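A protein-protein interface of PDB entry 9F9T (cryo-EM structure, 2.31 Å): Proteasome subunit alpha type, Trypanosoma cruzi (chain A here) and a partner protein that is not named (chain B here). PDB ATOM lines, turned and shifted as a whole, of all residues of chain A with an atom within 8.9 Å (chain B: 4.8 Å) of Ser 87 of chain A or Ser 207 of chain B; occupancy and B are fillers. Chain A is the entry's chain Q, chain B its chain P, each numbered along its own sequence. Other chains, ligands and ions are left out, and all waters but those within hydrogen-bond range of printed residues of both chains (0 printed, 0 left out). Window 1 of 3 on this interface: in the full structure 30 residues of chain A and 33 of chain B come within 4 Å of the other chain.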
ATOM      1  N   TYR A  72      14.686  24.609  -4.015  1.00  0.00           N
ATOM      2  CA  TYR A  72      13.716  23.773  -4.680  1.00  0.00           C
ATOM      3  C   TYR A  72      12.340  24.413  -4.630  1.00  0.00           C
ATOM      4  O   TYR A  72      11.908  24.926  -3.623  1.00  0.00           O
ATOM      5  CB  TYR A  72      13.707  22.405  -4.032  1.00  0.00           C
ATOM      6  CG  TYR A  72      15.074  21.759  -4.042  1.00  0.00           C
ATOM      7  CD1 TYR A  72      15.526  21.051  -5.145  1.00  0.00           C
ATOM      8  CD2 TYR A  72      15.899  21.838  -2.933  1.00  0.00           C
ATOM      9  CE1 TYR A  72      16.789  20.480  -5.149  1.00  0.00           C
ATOM     10  CE2 TYR A  72      17.166  21.285  -2.934  1.00  0.00           C
ATOM     11  CZ  TYR A  72      17.629  20.633  -4.058  1.00  0.00           C
ATOM     12  OH  TYR A  72      18.889  20.087  -4.045  1.00  0.00           O
ATOM     13  N   VAL A  82      17.787  23.769   1.824  1.00  0.00           N
ATOM     14  CA  VAL A  82      18.038  22.679   2.743  1.00  0.00           C
ATOM     15  C   VAL A  82      19.448  22.844   3.229  1.00  0.00           C
ATOM     16  O   VAL A  82      20.253  23.392   2.492  1.00  0.00           O
ATOM     17  CB  VAL A  82      17.929  21.292   2.096  1.00  0.00           C
ATOM     18  CG1 VAL A  82      16.648  21.123   1.298  1.00  0.00           C
ATOM     19  CG2 VAL A  82      19.134  20.996   1.217  1.00  0.00           C
ATOM     20  N   GLY A  84      22.159  19.927   5.358  1.00  0.00           N
ATOM     21  CA  GLY A  84      22.230  18.578   5.895  1.00  0.00           C
ATOM     22  C   GLY A  84      22.288  17.510   4.816  1.00  0.00           C
ATOM     23  O   GLY A  84      22.644  17.813   3.681  1.00  0.00           O
ATOM     24  N   VAL A  85      21.950  16.262   5.180  1.00  0.00           N
ATOM     25  CA  VAL A  85      22.166  15.098   4.317  1.00  0.00           C
ATOM     26  C   VAL A  85      21.347  15.209   3.015  1.00  0.00           C
ATOM     27  O   VAL A  85      20.139  14.969   2.996  1.00  0.00           O
ATOM     28  CB  VAL A  85      21.894  13.774   5.083  1.00  0.00           C
ATOM     29  CG1 VAL A  85      22.021  12.538   4.181  1.00  0.00           C
ATOM     30  CG2 VAL A  85      22.792  13.597   6.321  1.00  0.00           C
ATOM     31  N   THR A  86      22.032  15.445   1.881  1.00  0.00           N
ATOM     32  CA  THR A  86      21.364  15.782   0.622  1.00  0.00           C
ATOM     33  C   THR A  86      20.271  14.776   0.222  1.00  0.00           C
ATOM     34  O   THR A  86      19.152  15.176  -0.108  1.00  0.00           O
ATOM     35  CB  THR A  86      22.339  15.875  -0.558  1.00  0.00           C
ATOM     36  OG1 THR A  86      23.446  16.729  -0.244  1.00  0.00           O
ATOM     37  CG2 THR A  86      21.613  16.336  -1.812  1.00  0.00           C
ATOM     38  N   SER A  87      20.595  13.478   0.229  1.00  0.00           N
ATOM     39  CA  SER A  87      19.634  12.443  -0.162  1.00  0.00           C
ATOM     40  C   SER A  87      18.411  12.392   0.774  1.00  0.00           C
ATOM     41  O   SER A  87      17.278  12.160   0.332  1.00  0.00           O
ATOM     42  CB  SER A  87      20.314  11.086  -0.237  1.00  0.00           C
ATOM     43  OG  SER A  87      19.563  10.158  -1.001  1.00  0.00           O
ATOM     44  N   ASP A  88      18.636  12.688   2.069  1.00  0.00           N
ATOM     45  CA  ASP A  88      17.546  12.822   3.030  1.00  0.00           C
ATOM     46  C   ASP A  88      16.660  13.983   2.610  1.00  0.00           C
ATOM     47  O   ASP A  88      15.445  13.785   2.551  1.00  0.00           O
ATOM     48  CB  ASP A  88      18.050  12.943   4.476  1.00  0.00           C
ATOM     49  CG  ASP A  88      18.433  11.596   5.086  1.00  0.00           C
ATOM     50  OD1 ASP A  88      18.278  10.588   4.372  1.00  0.00           O
ATOM     51  OD2 ASP A  88      18.831  11.550   6.291  1.00  0.00           O
ATOM     52  N   ALA A  89      17.262  15.109   2.191  1.00  0.00           N
ATOM     53  CA  ALA A  89      16.443  16.222   1.723  1.00  0.00           C
ATOM     54  C   ALA A  89      15.549  15.849   0.540  1.00  0.00           C
ATOM     55  O   ALA A  89      14.391  16.220   0.538  1.00  0.00           O
ATOM     56  CB  ALA A  89      17.265  17.416   1.361  1.00  0.00           C
ATOM     57  N   TYR A  90      16.061  15.101  -0.438  1.00  0.00           N
ATOM     58  CA  TYR A  90      15.290  14.708  -1.612  1.00  0.00           C
ATOM     59  C   TYR A  90      14.129  13.815  -1.198  1.00  0.00           C
ATOM     60  O   TYR A  90      13.042  13.990  -1.727  1.00  0.00           O
ATOM     61  CB  TYR A  90      16.039  13.972  -2.732  1.00  0.00           C
ATOM     62  CG  TYR A  90      17.127  14.746  -3.462  1.00  0.00           C
ATOM     63  CD1 TYR A  90      16.987  16.086  -3.785  1.00  0.00           C
ATOM     64  CD2 TYR A  90      18.305  14.117  -3.863  1.00  0.00           C
ATOM     65  CE1 TYR A  90      17.967  16.778  -4.475  1.00  0.00           C
ATOM     66  CE2 TYR A  90      19.309  14.801  -4.532  1.00  0.00           C
ATOM     67  CZ  TYR A  90      19.134  16.137  -4.850  1.00  0.00           C
ATOM     68  OH  TYR A  90      20.118  16.829  -5.511  1.00  0.00           O
ATOM     69  N   ALA A  91      14.306  12.875  -0.266  1.00  0.00           N
ATOM     70  CA  ALA A  91      13.132  12.119   0.174  1.00  0.00           C
ATOM     71  C   ALA A  91      12.046  13.009   0.778  1.00  0.00           C
ATOM     72  O   ALA A  91      10.866  12.768   0.539  1.00  0.00           O
ATOM     73  CB  ALA A  91      13.465  11.037   1.145  1.00  0.00           C
ATOM     74  N   LEU A  92      12.407  14.036   1.528  1.00  0.00           N
ATOM     75  CA  LEU A  92      11.389  14.834   2.158  1.00  0.00           C
ATOM     76  C   LEU A  92      10.782  15.819   1.186  1.00  0.00           C
ATOM     77  O   LEU A  92       9.612  16.172   1.300  1.00  0.00           O
ATOM     78  CB  LEU A  92      11.999  15.620   3.322  1.00  0.00           C
ATOM     79  CG  LEU A  92      12.168  14.830   4.605  1.00  0.00           C
ATOM     80  CD1 LEU A  92      12.498  15.771   5.732  1.00  0.00           C
ATOM     81  CD2 LEU A  92      10.895  14.050   4.925  1.00  0.00           C
ATOM     82  N   LEU A  93      11.592  16.334   0.279  1.00  0.00           N
ATOM     83  CA  LEU A  93      11.051  17.223  -0.739  1.00  0.00           C
ATOM     84  C   LEU A  93      10.009  16.506  -1.638  1.00  0.00           C
ATOM     85  O   LEU A  93       8.979  17.076  -1.958  1.00  0.00           O
ATOM     86  CB  LEU A  93      12.261  17.761  -1.501  1.00  0.00           C
ATOM     87  CG  LEU A  93      11.937  18.537  -2.771  1.00  0.00           C
ATOM     88  CD1 LEU A  93      11.654  19.966  -2.374  1.00  0.00           C
ATOM     89  CD2 LEU A  93      13.082  18.452  -3.817  1.00  0.00           C
ATOM     90  N   ASN A  94      10.203  15.233  -1.979  1.00  0.00           N
ATOM     91  CA  ASN A  94       9.157  14.476  -2.636  1.00  0.00           C
ATOM     92  C   ASN A  94       7.918  14.396  -1.746  1.00  0.00           C
ATOM     93  O   ASN A  94       6.811  14.616  -2.196  1.00  0.00           O
ATOM     94  CB  ASN A  94       9.669  13.135  -3.174  1.00  0.00           C
ATOM     95  CG  ASN A  94      10.824  13.306  -4.169  1.00  0.00           C
ATOM     96  OD1 ASN A  94      11.894  12.708  -4.026  1.00  0.00           O
ATOM     97  ND2 ASN A  94      10.638  14.135  -5.192  1.00  0.00           N
ATOM     98  N   ARG A 134      17.191   5.437  11.955  1.00  0.00           N
ATOM     99  CA  ARG A 134      17.675   6.799  12.195  1.00  0.00           C
ATOM    100  C   ARG A 134      16.626   7.812  11.765  1.00  0.00           C
ATOM    101  O   ARG A 134      15.743   7.515  10.947  1.00  0.00           O
ATOM    102  CB  ARG A 134      18.991   7.151  11.505  1.00  0.00           C
ATOM    103  CG  ARG A 134      18.947   7.196   9.986  1.00  0.00           C
ATOM    104  CD  ARG A 134      20.303   7.637   9.437  1.00  0.00           C
ATOM    105  NE  ARG A 134      20.323   7.613   7.982  1.00  0.00           N
ATOM    106  CZ  ARG A 134      19.824   8.565   7.208  1.00  0.00           C
ATOM    107  NH1 ARG A 134      19.406   9.682   7.768  1.00  0.00           N
ATOM    108  NH2 ARG A 134      19.774   8.406   5.892  1.00  0.00           N
ATOM    109  N   PHE A 136      15.677  11.595   9.860  1.00  0.00           N
ATOM    110  CA  PHE A 136      16.137  12.441   8.764  1.00  0.00           C
ATOM    111  C   PHE A 136      17.061  13.525   9.312  1.00  0.00           C
ATOM    112  O   PHE A 136      16.703  14.214  10.265  1.00  0.00           O
ATOM    113  CB  PHE A 136      14.971  13.090   8.006  1.00  0.00           C
ATOM    114  CG  PHE A 136      14.103  12.121   7.246  1.00  0.00           C
ATOM    115  CD1 PHE A 136      14.589  11.466   6.118  1.00  0.00           C
ATOM    116  CD2 PHE A 136      12.808  11.850   7.661  1.00  0.00           C
ATOM    117  CE1 PHE A 136      13.790  10.586   5.399  1.00  0.00           C
ATOM    118  CE2 PHE A 136      12.012  10.965   6.947  1.00  0.00           C
ATOM    119  CZ  PHE A 136      12.506  10.329   5.826  1.00  0.00           C
ATOM    120  N   GLY A 137      18.217  13.679   8.656  1.00  0.00           N
ATOM    121  CA  GLY A 137      19.234  14.641   9.067  1.00  0.00           C
ATOM    122  C   GLY A 137      19.184  15.933   8.259  1.00  0.00           C
ATOM    123  O   GLY A 137      20.215  16.368   7.775  1.00  0.00           O
ATOM    124  N   VAL A 138      18.009  16.575   8.222  1.00  0.00           N
ATOM    125  CA  VAL A 138      17.779  17.753   7.389  1.00  0.00           C
ATOM    126  C   VAL A 138      17.179  18.926   8.163  1.00  0.00           C
ATOM    127  O   VAL A 138      16.353  18.740   9.044  1.00  0.00           O
ATOM    128  CB  VAL A 138      16.842  17.383   6.232  1.00  0.00           C
ATOM    129  CG1 VAL A 138      16.659  18.542   5.285  1.00  0.00           C
ATOM    130  CG2 VAL A 138      17.381  16.163   5.507  1.00  0.00           C
ATOM    131  N   PHE A 140      15.136  22.634   6.993  1.00  0.00           N
ATOM    132  CA  PHE A 140      14.628  23.345   5.830  1.00  0.00           C
ATOM    133  C   PHE A 140      14.369  24.808   6.143  1.00  0.00           C
ATOM    134  O   PHE A 140      13.955  25.108   7.245  1.00  0.00           O
ATOM    135  CB  PHE A 140      13.246  22.842   5.396  1.00  0.00           C
ATOM    136  CG  PHE A 140      13.195  21.526   4.660  1.00  0.00           C
ATOM    137  CD1 PHE A 140      12.954  21.488   3.293  1.00  0.00           C
ATOM    138  CD2 PHE A 140      13.370  20.328   5.326  1.00  0.00           C
ATOM    139  CE1 PHE A 140      12.902  20.282   2.605  1.00  0.00           C
ATOM    140  CE2 PHE A 140      13.320  19.121   4.640  1.00  0.00           C
ATOM    141  CZ  PHE A 140      13.073  19.097   3.284  1.00  0.00           C
ATOM    142  N   ILE B  77      27.978   4.829   6.013  1.00  0.00           N
ATOM    143  CA  ILE B  77      28.016   5.442   4.704  1.00  0.00           C
ATOM    144  C   ILE B  77      29.424   5.835   4.315  1.00  0.00           C
ATOM    145  O   ILE B  77      29.666   5.905   3.117  1.00  0.00           O
ATOM    146  CB  ILE B  77      27.084   6.662   4.597  1.00  0.00           C
ATOM    147  CG1 ILE B  77      25.626   6.241   4.713  1.00  0.00           C
ATOM    148  CG2 ILE B  77      27.341   7.388   3.281  1.00  0.00           C
ATOM    149  CD1 ILE B  77      24.658   7.425   4.708  1.00  0.00           C
ATOM    150  N   SER B 170      19.550   6.970  -7.043  1.00  0.00           N
ATOM    151  CA  SER B 170      19.801   7.730  -5.831  1.00  0.00           C
ATOM    152  C   SER B 170      18.871   7.356  -4.695  1.00  0.00           C
ATOM    153  O   SER B 170      19.307   7.199  -3.570  1.00  0.00           O
ATOM    154  CB  SER B 170      19.589   9.176  -6.150  1.00  0.00           C
ATOM    155  OG  SER B 170      20.415   9.993  -5.376  1.00  0.00           O
ATOM    156  N   TYR B 173      19.570   4.039  -3.452  1.00  0.00           N
ATOM    157  CA  TYR B 173      20.726   4.017  -2.565  1.00  0.00           C
ATOM    158  C   TYR B 173      20.311   4.542  -1.188  1.00  0.00           C
ATOM    159  O   TYR B 173      20.821   4.056  -0.191  1.00  0.00           O
ATOM    160  CB  TYR B 173      21.834   4.965  -2.987  1.00  0.00           C
ATOM    161  CG  TYR B 173      22.889   4.485  -3.943  1.00  0.00           C
ATOM    162  CD1 TYR B 173      23.963   3.777  -3.490  1.00  0.00           C
ATOM    163  CD2 TYR B 173      22.886   4.817  -5.277  1.00  0.00           C
ATOM    164  CE1 TYR B 173      24.995   3.358  -4.312  1.00  0.00           C
ATOM    165  CE2 TYR B 173      23.902   4.394  -6.130  1.00  0.00           C
ATOM    166  CZ  TYR B 173      24.991   3.707  -5.633  1.00  0.00           C
ATOM    167  OH  TYR B 173      26.026   3.293  -6.402  1.00  0.00           O
ATOM    168  N   GLN B 174      19.446   5.571  -1.167  1.00  0.00           N
ATOM    169  CA  GLN B 174      19.147   6.325   0.027  1.00  0.00           C
ATOM    170  C   GLN B 174      18.282   5.483   0.956  1.00  0.00           C
ATOM    171  O   GLN B 174      18.338   5.686   2.155  1.00  0.00           O
ATOM    172  CB  GLN B 174      18.327   7.591  -0.260  1.00  0.00           C
ATOM    173  CG  GLN B 174      18.109   8.520   0.950  1.00  0.00           C
ATOM    174  CD  GLN B 174      16.983   8.216   1.938  1.00  0.00           C
ATOM    175  OE1 GLN B 174      15.974   7.586   1.647  1.00  0.00           O
ATOM    176  NE2 GLN B 174      17.098   8.769   3.131  1.00  0.00           N
ATOM    177  N   THR B 177      20.175   3.351   3.378  1.00  0.00           N
ATOM    178  CA  THR B 177      20.928   4.043   4.430  1.00  0.00           C
ATOM    179  C   THR B 177      20.024   4.421   5.610  1.00  0.00           C
ATOM    180  O   THR B 177      20.489   5.083   6.532  1.00  0.00           O
ATOM    181  CB  THR B 177      21.561   5.384   3.995  1.00  0.00           C
ATOM    182  OG1 THR B 177      20.610   6.303   3.480  1.00  0.00           O
ATOM    183  CG2 THR B 177      22.615   5.259   2.929  1.00  0.00           C
ATOM    184  N   ASP B 205      26.988   8.069  -5.685  1.00  0.00           N
ATOM    185  CA  ASP B 205      27.813   7.523  -4.635  1.00  0.00           C
ATOM    186  C   ASP B 205      26.952   6.783  -3.637  1.00  0.00           C
ATOM    187  O   ASP B 205      25.752   7.033  -3.543  1.00  0.00           O
ATOM    188  CB  ASP B 205      28.622   8.667  -4.055  1.00  0.00           C
ATOM    189  CG  ASP B 205      30.040   8.707  -4.661  1.00  0.00           C
ATOM    190  OD1 ASP B 205      30.226   8.108  -5.816  1.00  0.00           O
ATOM    191  OD2 ASP B 205      31.018   9.255  -3.958  1.00  0.00           O
ATOM    192  N   PRO B 206      27.527   5.888  -2.810  1.00  0.00           N
ATOM    193  CA  PRO B 206      26.780   5.221  -1.739  1.00  0.00           C
ATOM    194  C   PRO B 206      25.864   6.027  -0.832  1.00  0.00           C
ATOM    195  O   PRO B 206      24.858   5.505  -0.404  1.00  0.00           O
ATOM    196  CB  PRO B 206      27.874   4.752  -0.813  1.00  0.00           C
ATOM    197  CG  PRO B 206      28.926   4.370  -1.838  1.00  0.00           C
ATOM    198  CD  PRO B 206      28.970   5.585  -2.756  1.00  0.00           C
ATOM    199  N   SER B 207      26.140   7.316  -0.666  1.00  0.00           N
ATOM    200  CA  SER B 207      25.244   8.194   0.065  1.00  0.00           C
ATOM    201  C   SER B 207      23.939   8.440  -0.654  1.00  0.00           C
ATOM    202  O   SER B 207      22.984   8.857  -0.046  1.00  0.00           O
ATOM    203  CB  SER B 207      25.904   9.530   0.317  1.00  0.00           C
ATOM    204  OG  SER B 207      25.954  10.346  -0.850  1.00  0.00           O
ATOM    205  N   GLY B 208      23.909   8.195  -1.969  1.00  0.00           N
ATOM    206  CA  GLY B 208      22.799   8.602  -2.802  1.00  0.00           C
ATOM    207  C   GLY B 208      23.014  10.003  -3.370  1.00  0.00           C
ATOM    208  O   GLY B 208      22.115  10.584  -3.938  1.00  0.00           O
ATOM    209  N   THR B 209      24.208  10.552  -3.273  1.00  0.00           N
ATOM    210  CA  THR B 209      24.428  11.845  -3.883  1.00  0.00           C
ATOM    211  C   THR B 209      24.911  11.652  -5.329  1.00  0.00           C
ATOM    212  O   THR B 209      25.718  10.784  -5.608  1.00  0.00           O
ATOM    213  CB  THR B 209      25.357  12.709  -3.030  1.00  0.00           C
ATOM    214  OG1 THR B 209      24.648  13.281  -1.930  1.00  0.00           O
ATOM    215  CG2 THR B 209      25.805  13.913  -3.804  1.00  0.00           C
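The backbone carbonyl oxygen (O) of Thr 177 of chain B sits at hydrogen-bond distance from the guanidinium group (NE) of Arg 134 of chain A.
The side-chain carboxylate (OD1) of Asp 88 of chain A sits at hydrogen-bond distance from the side-chain amide nitrogen (NE2) of Gln 174 of chain B (2.5 Å).
The side-chain carboxylate (OD2) of Asp 88 of chain A is in hydrogen-bond range of the backbone NH (N) of Gly 137 of chain A (3.2 Å).
OD2 of Asp 88 of chain A is in salt-bridge range of NH1 of Arg 134 of chain A (2.4 Å).
OG of Ser 207 of chain B sits at hydrogen-bond distance from N of Thr 209 of chain B, at 3.0 Å.
The side-chain hydroxyl of Thr 177 of chain B sits at hydrogen-bond distance from the backbone carbonyl oxygen of Gln 174 of chain B (2.7 Å).
Thr 86 of chain A touches Thr 209 of chain B.
OG of Ser 87 of chain A touches O of Ser 170 of chain B (3.9 Å).
Ser 87 of chain A touches Gln 174 of chain B (OG to CG, 2.9 Å).
CB of Ser 87 of chain A touches O of Ser 207 of chain B, at 3.5 Å.
Gly 208 of chain B touches Ser 87 of chain A (O to OG, 3.9 Å).
Gln 174 of chain B touches Arg 134 of chain A.
Ser 87 of chain A touches four residues of chain B.
Of the printed residues of chain A, Ser 207 of chain B touches Ser 87 (3.5 Å).
Gly 208 of chain B touches just one residue of chain A: Ser 87.
Of chain A, only Thr 86 (3.7 Å) comes within 4 Å of Thr 209 of chain B.
Of the printed residues of chain B, Asp 88 of chain A touches Gln 174 (2.5 Å).
Of the printed residues of chain A, Thr 177 of chain B touches Arg 134 (2.9 Å).
Printed residues of chain B within 4 Å of Arg 134 of chain A: Gln 174 and Thr 177.
Printed residues of chain A within 4 Å of Ser 170 of chain B: Ser 87.
Of the printed residues of chain A, Gln 174 of chain B touches Ser 87, Asp 88 and Arg 134.
Phe 140 of chain A touches none of the printed residues of chain B.
The nearest residue of chain B that does not touch Ser 87 of chain A is Thr 209 of chain B (4.6 Å).
The nearest residue of chain A that does not touch Ser 207 of chain B is Val 85 of chain A (5.7 Å).
Of the 10 printed residues of chain B, 6 touch a printed residue of chain A.
Of the 18 printed residues of chain A, 4 touch a printed residue of chain B.
Printed residues of chain A that touch a printed residue of chain B: Thr 86, Ser 87, Asp 88 and Arg 134.
Along chain A the printed residues that touch a printed residue of chain B span positions 86 to 134.
Among the printed residues, no Asp or Glu carboxylate lies within 4 Å of a Lys or Arg side-chain nitrogen of the other chain.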
